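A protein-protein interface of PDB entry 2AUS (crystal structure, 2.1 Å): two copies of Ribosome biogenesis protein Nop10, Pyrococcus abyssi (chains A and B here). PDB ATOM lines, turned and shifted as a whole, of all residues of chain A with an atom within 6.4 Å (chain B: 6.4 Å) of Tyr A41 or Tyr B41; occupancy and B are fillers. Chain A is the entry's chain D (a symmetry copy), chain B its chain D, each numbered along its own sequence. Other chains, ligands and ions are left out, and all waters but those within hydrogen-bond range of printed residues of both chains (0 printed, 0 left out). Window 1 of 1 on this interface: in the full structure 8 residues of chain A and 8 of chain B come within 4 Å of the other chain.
OD1 of Asp B39 lies within salt-bridge range of NH1 of Arg B45 (2.6 Å).
OD1 of Asp A39 lies within salt-bridge range of NH1 of Arg A45 (2.6 Å).
Tyr A41 touches Tyr B41 (CD2 to CD2, 3.2 Å).
CD2 of Tyr B44 touches CE1 of Tyr A41 (3.7 Å).
Tyr A41 touches Arg B45 (OH to CB, 3.6 Å).
Tyr B41 touches Tyr A44 (CE1 to CD2, 3.7 Å).
Tyr A44 touches Tyr B44.
Tyr B41 touches Arg A45.
Tyr A41 touches three residues of chain B.
Of the printed residues of chain B, Tyr A44 touches Tyr B41 and Tyr B44.
Of the printed residues of chain B, Arg A45 touches Tyr B41 (3.5 Å).
Tyr B41 touches three residues of chain A.
Leu B48 touches none of the printed residues of chain A.
Of the 10 printed residues of chain A, 3 touch a printed residue of chain B.
Printed residues of chain A that touch a printed residue of chain B: Tyr A41, Tyr A44 and Arg A45.
Hydrophobic or aromatic side chains of chain A within 4 Å of the printed part of chain B: Tyr A41 and Tyr A44.
Among the printed residues, no Asp or Glu carboxylate lies within 4 Å of a Lys or Arg side-chain nitrogen of the other chain.
Tyr B41 touches its own counterpart, Tyr A41.
Tyr A41 touches Tyr B44, and with the chains exchanged Tyr A44 touches Tyr B41.
Tyr A41 touches Arg B45, and with the chains exchanged Arg A45 touches Tyr B41.
Tyr B44 touches its own counterpart, Tyr A44.
Positions printed for both chains: 38, 39, 40, 41, 42, 43, 44, 45, 46 and 48.
Of the 6 pairs that touch across the chains among the printed residues, 6 have their exchanged pair printed and touching as well.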
ATOM      1  N   GLU A  38       7.702   0.911 -11.402  1.00  0.00           N
ATOM      2  CA  GLU A  38       7.526   1.149  -9.972  1.00  0.00           C
ATOM      3  C   GLU A  38       6.865  -0.059  -9.316  1.00  0.00           C
ATOM      4  O   GLU A  38       7.465  -0.720  -8.471  1.00  0.00           O
ATOM      5  CB  GLU A  38       6.671   2.397  -9.735  1.00  0.00           C
ATOM      6  CG  GLU A  38       7.293   3.695 -10.238  1.00  0.00           C
ATOM      7  CD  GLU A  38       6.483   4.920  -9.839  1.00  0.00           C
ATOM      8  OE1 GLU A  38       5.287   4.992 -10.202  1.00  0.00           O
ATOM      9  OE2 GLU A  38       7.040   5.816  -9.167  1.00  0.00           O
ATOM     10  N   ASP A  39       5.627  -0.341  -9.705  1.00  0.00           N
ATOM     11  CA  ASP A  39       4.900  -1.479  -9.155  1.00  0.00           C
ATOM     12  C   ASP A  39       4.853  -1.422  -7.623  1.00  0.00           C
ATOM     13  O   ASP A  39       5.317  -2.333  -6.936  1.00  0.00           O
ATOM     14  CB  ASP A  39       5.566  -2.775  -9.625  1.00  0.00           C
ATOM     15  CG  ASP A  39       4.710  -3.992  -9.381  1.00  0.00           C
ATOM     16  OD1 ASP A  39       3.481  -3.883  -9.577  1.00  0.00           O
ATOM     17  OD2 ASP A  39       5.269  -5.049  -9.004  1.00  0.00           O
ATOM     18  N   PRO A  40       4.272  -0.343  -7.072  1.00  0.00           N
ATOM     19  CA  PRO A  40       4.139  -0.111  -5.629  1.00  0.00           C
ATOM     20  C   PRO A  40       3.389  -1.208  -4.875  1.00  0.00           C
ATOM     21  O   PRO A  40       3.703  -1.509  -3.724  1.00  0.00           O
ATOM     22  CB  PRO A  40       3.390   1.222  -5.559  1.00  0.00           C
ATOM     23  CG  PRO A  40       3.745   1.891  -6.859  1.00  0.00           C
ATOM     24  CD  PRO A  40       3.650   0.755  -7.829  1.00  0.00           C
ATOM     25  N   TYR A  41       2.392  -1.796  -5.529  1.00  0.00           N
ATOM     26  CA  TYR A  41       1.581  -2.834  -4.910  1.00  0.00           C
ATOM     27  C   TYR A  41       2.060  -4.246  -5.227  1.00  0.00           C
ATOM     28  O   TYR A  41       1.368  -5.224  -4.928  1.00  0.00           O
ATOM     29  CB  TYR A  41       0.121  -2.665  -5.343  1.00  0.00           C
ATOM     30  CG  TYR A  41      -0.472  -1.330  -4.940  1.00  0.00           C
ATOM     31  CD1 TYR A  41      -0.879  -1.091  -3.626  1.00  0.00           C
ATOM     32  CD2 TYR A  41      -0.595  -0.294  -5.865  1.00  0.00           C
ATOM     33  CE1 TYR A  41      -1.395   0.145  -3.245  1.00  0.00           C
ATOM     34  CE2 TYR A  41      -1.105   0.943  -5.493  1.00  0.00           C
ATOM     35  CZ  TYR A  41      -1.504   1.158  -4.184  1.00  0.00           C
ATOM     36  OH  TYR A  41      -2.012   2.383  -3.814  1.00  0.00           O
ATOM     37  N   GLY A  42       3.245  -4.346  -5.827  1.00  0.00           N
ATOM     38  CA  GLY A  42       3.800  -5.646  -6.165  1.00  0.00           C
ATOM     39  C   GLY A  42       3.793  -6.598  -4.982  1.00  0.00           C
ATOM     40  O   GLY A  42       3.339  -7.735  -5.091  1.00  0.00           O
ATOM     41  N   GLU A  43       4.291  -6.135  -3.841  1.00  0.00           N
ATOM     42  CA  GLU A  43       4.327  -6.975  -2.651  1.00  0.00           C
ATOM     43  C   GLU A  43       2.914  -7.322  -2.219  1.00  0.00           C
ATOM     44  O   GLU A  43       2.644  -8.438  -1.781  1.00  0.00           O
ATOM     45  CB  GLU A  43       5.070  -6.265  -1.514  1.00  0.00           C
ATOM     46  CG  GLU A  43       6.542  -6.006  -1.830  1.00  0.00           C
ATOM     47  CD  GLU A  43       7.314  -5.438  -0.652  1.00  0.00           C
ATOM     48  OE1 GLU A  43       7.364  -6.104   0.409  1.00  0.00           O
ATOM     49  OE2 GLU A  43       7.882  -4.329  -0.795  1.00  0.00           O
ATOM     50  N   TYR A  44       2.005  -6.366  -2.364  1.00  0.00           N
ATOM     51  CA  TYR A  44       0.618  -6.586  -1.985  1.00  0.00           C
ATOM     52  C   TYR A  44      -0.063  -7.656  -2.835  1.00  0.00           C
ATOM     53  O   TYR A  44      -0.592  -8.638  -2.303  1.00  0.00           O
ATOM     54  CB  TYR A  44      -0.179  -5.280  -2.075  1.00  0.00           C
ATOM     55  CG  TYR A  44      -1.665  -5.481  -1.879  1.00  0.00           C
ATOM     56  CD1 TYR A  44      -2.166  -6.014  -0.690  1.00  0.00           C
ATOM     57  CD2 TYR A  44      -2.570  -5.167  -2.894  1.00  0.00           C
ATOM     58  CE1 TYR A  44      -3.533  -6.232  -0.518  1.00  0.00           C
ATOM     59  CE2 TYR A  44      -3.935  -5.383  -2.731  1.00  0.00           C
ATOM     60  CZ  TYR A  44      -4.408  -5.915  -1.542  1.00  0.00           C
ATOM     61  OH  TYR A  44      -5.755  -6.137  -1.382  1.00  0.00           O
ATOM     62  N   ARG A  45      -0.051  -7.485  -4.153  1.00  0.00           N
ATOM     63  CA  ARG A  45      -0.709  -8.480  -4.993  1.00  0.00           C
ATOM     64  C   ARG A  45      -0.017  -9.829  -4.909  1.00  0.00           C
ATOM     65  O   ARG A  45      -0.659 -10.866  -5.072  1.00  0.00           O
ATOM     66  CB  ARG A  45      -0.794  -8.026  -6.456  1.00  0.00           C
ATOM     67  CG  ARG A  45       0.507  -8.017  -7.183  1.00  0.00           C
ATOM     68  CD  ARG A  45       0.317  -8.178  -8.695  1.00  0.00           C
ATOM     69  NE  ARG A  45       1.628  -8.116  -9.319  1.00  0.00           N
ATOM     70  CZ  ARG A  45       2.342  -7.003  -9.409  1.00  0.00           C
ATOM     71  NH1 ARG A  45       1.850  -5.868  -8.936  1.00  0.00           N
ATOM     72  NH2 ARG A  45       3.570  -7.038  -9.906  1.00  0.00           N
ATOM     73  N   ARG A  46       1.287  -9.829  -4.653  1.00  0.00           N
ATOM     74  CA  ARG A  46       1.996 -11.098  -4.531  1.00  0.00           C
ATOM     75  C   ARG A  46       1.497 -11.835  -3.296  1.00  0.00           C
ATOM     76  O   ARG A  46       1.423 -13.063  -3.285  1.00  0.00           O
ATOM     77  CB  ARG A  46       3.510 -10.887  -4.438  1.00  0.00           C
ATOM     78  CG  ARG A  46       4.198 -10.889  -5.793  1.00  0.00           C
ATOM     79  CD  ARG A  46       5.690 -11.064  -5.660  1.00  0.00           C
ATOM     80  NE  ARG A  46       6.364  -9.849  -5.215  1.00  0.00           N
ATOM     81  CZ  ARG A  46       6.444  -8.733  -5.930  1.00  0.00           C
ATOM     82  NH1 ARG A  46       5.884  -8.668  -7.128  1.00  0.00           N
ATOM     83  NH2 ARG A  46       7.105  -7.686  -5.456  1.00  0.00           N
ATOM     84  N   LEU A  48      -1.486 -11.708  -2.210  1.00  0.00           N
ATOM     85  CA  LEU A  48      -2.807 -12.219  -2.564  1.00  0.00           C
ATOM     86  C   LEU A  48      -2.664 -13.527  -3.341  1.00  0.00           C
ATOM     87  O   LEU A  48      -3.455 -14.453  -3.166  1.00  0.00           O
ATOM     88  CB  LEU A  48      -3.570 -11.192  -3.408  1.00  0.00           C
ATOM     89  CG  LEU A  48      -4.014  -9.905  -2.699  1.00  0.00           C
ATOM     90  CD1 LEU A  48      -4.566  -8.913  -3.720  1.00  0.00           C
ATOM     91  CD2 LEU A  48      -5.066 -10.239  -1.644  1.00  0.00           C
ATOM     92  N   GLU B  38      -6.947   4.193 -14.650  1.00  0.00           N
ATOM     93  CA  GLU B  38      -7.430   2.901 -14.173  1.00  0.00           C
ATOM     94  C   GLU B  38      -7.522   2.904 -12.651  1.00  0.00           C
ATOM     95  O   GLU B  38      -8.609   2.786 -12.088  1.00  0.00           O
ATOM     96  CB  GLU B  38      -6.498   1.775 -14.631  1.00  0.00           C
ATOM     97  CG  GLU B  38      -6.424   1.591 -16.143  1.00  0.00           C
ATOM     98  CD  GLU B  38      -5.615   0.364 -16.540  1.00  0.00           C
ATOM     99  OE1 GLU B  38      -4.424   0.284 -16.162  1.00  0.00           O
ATOM    100  OE2 GLU B  38      -6.164  -0.519 -17.234  1.00  0.00           O
ATOM    101  N   ASP B  39      -6.378   3.034 -11.988  1.00  0.00           N
ATOM    102  CA  ASP B  39      -6.345   3.063 -10.531  1.00  0.00           C
ATOM    103  C   ASP B  39      -7.034   1.829  -9.935  1.00  0.00           C
ATOM    104  O   ASP B  39      -7.998   1.940  -9.175  1.00  0.00           O
ATOM    105  CB  ASP B  39      -7.020   4.346 -10.037  1.00  0.00           C
ATOM    106  CG  ASP B  39      -6.752   4.622  -8.580  1.00  0.00           C
ATOM    107  OD1 ASP B  39      -5.604   4.382  -8.147  1.00  0.00           O
ATOM    108  OD2 ASP B  39      -7.683   5.083  -7.879  1.00  0.00           O
ATOM    109  N   PRO B  40      -6.528   0.629 -10.267  1.00  0.00           N
ATOM    110  CA  PRO B  40      -7.055  -0.658  -9.801  1.00  0.00           C
ATOM    111  C   PRO B  40      -7.090  -0.819  -8.282  1.00  0.00           C
ATOM    112  O   PRO B  40      -7.991  -1.455  -7.737  1.00  0.00           O
ATOM    113  CB  PRO B  40      -6.108  -1.675 -10.444  1.00  0.00           C
ATOM    114  CG  PRO B  40      -5.593  -0.953 -11.659  1.00  0.00           C
ATOM    115  CD  PRO B  40      -5.349   0.423 -11.123  1.00  0.00           C
ATOM    116  N   TYR B  41      -6.102  -0.243  -7.606  1.00  0.00           N
ATOM    117  CA  TYR B  41      -6.005  -0.348  -6.158  1.00  0.00           C
ATOM    118  C   TYR B  41      -6.628   0.833  -5.422  1.00  0.00           C
ATOM    119  O   TYR B  41      -6.461   0.973  -4.207  1.00  0.00           O
ATOM    120  CB  TYR B  41      -4.535  -0.500  -5.755  1.00  0.00           C
ATOM    121  CG  TYR B  41      -3.879  -1.734  -6.341  1.00  0.00           C
ATOM    122  CD1 TYR B  41      -4.113  -2.999  -5.799  1.00  0.00           C
ATOM    123  CD2 TYR B  41      -3.050  -1.641  -7.458  1.00  0.00           C
ATOM    124  CE1 TYR B  41      -3.537  -4.139  -6.354  1.00  0.00           C
ATOM    125  CE2 TYR B  41      -2.473  -2.773  -8.021  1.00  0.00           C
ATOM    126  CZ  TYR B  41      -2.719  -4.018  -7.466  1.00  0.00           C
ATOM    127  OH  TYR B  41      -2.146  -5.141  -8.021  1.00  0.00           O
ATOM    128  N   GLY B  42      -7.351   1.673  -6.161  1.00  0.00           N
ATOM    129  CA  GLY B  42      -7.998   2.827  -5.558  1.00  0.00           C
ATOM    130  C   GLY B  42      -8.821   2.451  -4.339  1.00  0.00           C
ATOM    131  O   GLY B  42      -8.695   3.062  -3.280  1.00  0.00           O
ATOM    132  N   GLU B  43      -9.665   1.434  -4.480  1.00  0.00           N
ATOM    133  CA  GLU B  43     -10.497   1.000  -3.365  1.00  0.00           C
ATOM    134  C   GLU B  43      -9.623   0.484  -2.237  1.00  0.00           C
ATOM    135  O   GLU B  43      -9.911   0.709  -1.063  1.00  0.00           O
ATOM    136  CB  GLU B  43     -11.477  -0.088  -3.818  1.00  0.00           C
ATOM    137  CG  GLU B  43     -12.479   0.404  -4.860  1.00  0.00           C
ATOM    138  CD  GLU B  43     -13.541  -0.628  -5.201  1.00  0.00           C
ATOM    139  OE1 GLU B  43     -14.275  -1.057  -4.280  1.00  0.00           O
ATOM    140  OE2 GLU B  43     -13.647  -0.997  -6.395  1.00  0.00           O
ATOM    141  N   TYR B  44      -8.540  -0.194  -2.596  1.00  0.00           N
ATOM    142  CA  TYR B  44      -7.628  -0.734  -1.600  1.00  0.00           C
ATOM    143  C   TYR B  44      -6.937   0.354  -0.782  1.00  0.00           C
ATOM    144  O   TYR B  44      -7.018   0.360   0.451  1.00  0.00           O
ATOM    145  CB  TYR B  44      -6.571  -1.623  -2.262  1.00  0.00           C
ATOM    146  CG  TYR B  44      -5.483  -2.060  -1.307  1.00  0.00           C
ATOM    147  CD1 TYR B  44      -5.786  -2.812  -0.171  1.00  0.00           C
ATOM    148  CD2 TYR B  44      -4.154  -1.694  -1.520  1.00  0.00           C
ATOM    149  CE1 TYR B  44      -4.791  -3.188   0.731  1.00  0.00           C
ATOM    150  CE2 TYR B  44      -3.154  -2.063  -0.626  1.00  0.00           C
ATOM    151  CZ  TYR B  44      -3.480  -2.809   0.496  1.00  0.00           C
ATOM    152  OH  TYR B  44      -2.496  -3.167   1.386  1.00  0.00           O
ATOM    153  N   ARG B  45      -6.261   1.282  -1.451  1.00  0.00           N
ATOM    154  CA  ARG B  45      -5.573   2.325  -0.699  1.00  0.00           C
ATOM    155  C   ARG B  45      -6.552   3.216   0.046  1.00  0.00           C
ATOM    156  O   ARG B  45      -6.217   3.763   1.096  1.00  0.00           O
ATOM    157  CB  ARG B  45      -4.671   3.179  -1.600  1.00  0.00           C
ATOM    158  CG  ARG B  45      -5.399   4.087  -2.531  1.00  0.00           C
ATOM    159  CD  ARG B  45      -4.551   5.301  -2.924  1.00  0.00           C
ATOM    160  NE  ARG B  45      -5.322   6.102  -3.860  1.00  0.00           N
ATOM    161  CZ  ARG B  45      -5.575   5.727  -5.105  1.00  0.00           C
ATOM    162  NH1 ARG B  45      -5.090   4.580  -5.558  1.00  0.00           N
ATOM    163  NH2 ARG B  45      -6.365   6.462  -5.875  1.00  0.00           N
ATOM    164  N   ARG B  46      -7.761   3.367  -0.483  1.00  0.00           N
ATOM    165  CA  ARG B  46      -8.751   4.187   0.206  1.00  0.00           C
ATOM    166  C   ARG B  46      -9.132   3.516   1.519  1.00  0.00           C
ATOM    167  O   ARG B  46      -9.405   4.188   2.511  1.00  0.00           O
ATOM    168  CB  ARG B  46      -9.999   4.401  -0.654  1.00  0.00           C
ATOM    169  CG  ARG B  46      -9.915   5.638  -1.533  1.00  0.00           C
ATOM    170  CD  ARG B  46     -11.268   6.035  -2.067  1.00  0.00           C
ATOM    171  NE  ARG B  46     -11.720   5.177  -3.157  1.00  0.00           N
ATOM    172  CZ  ARG B  46     -11.140   5.116  -4.350  1.00  0.00           C
ATOM    173  NH1 ARG B  46     -10.076   5.858  -4.612  1.00  0.00           N
ATOM    174  NH2 ARG B  46     -11.640   4.328  -5.292  1.00  0.00           N
ATOM    175  N   LEU B  48      -7.142   1.801   3.305  1.00  0.00           N
ATOM    176  CA  LEU B  48      -6.008   2.013   4.199  1.00  0.00           C
ATOM    177  C   LEU B  48      -6.101   3.401   4.831  1.00  0.00           C
ATOM    178  O   LEU B  48      -5.776   3.582   6.005  1.00  0.00           O
ATOM    179  CB  LEU B  48      -4.688   1.877   3.432  1.00  0.00           C
ATOM    180  CG  LEU B  48      -4.317   0.473   2.935  1.00  0.00           C
ATOM    181  CD1 LEU B  48      -3.096   0.550   2.021  1.00  0.00           C
ATOM    182  CD2 LEU B  48      -4.043  -0.438   4.130  1.00  0.00           C
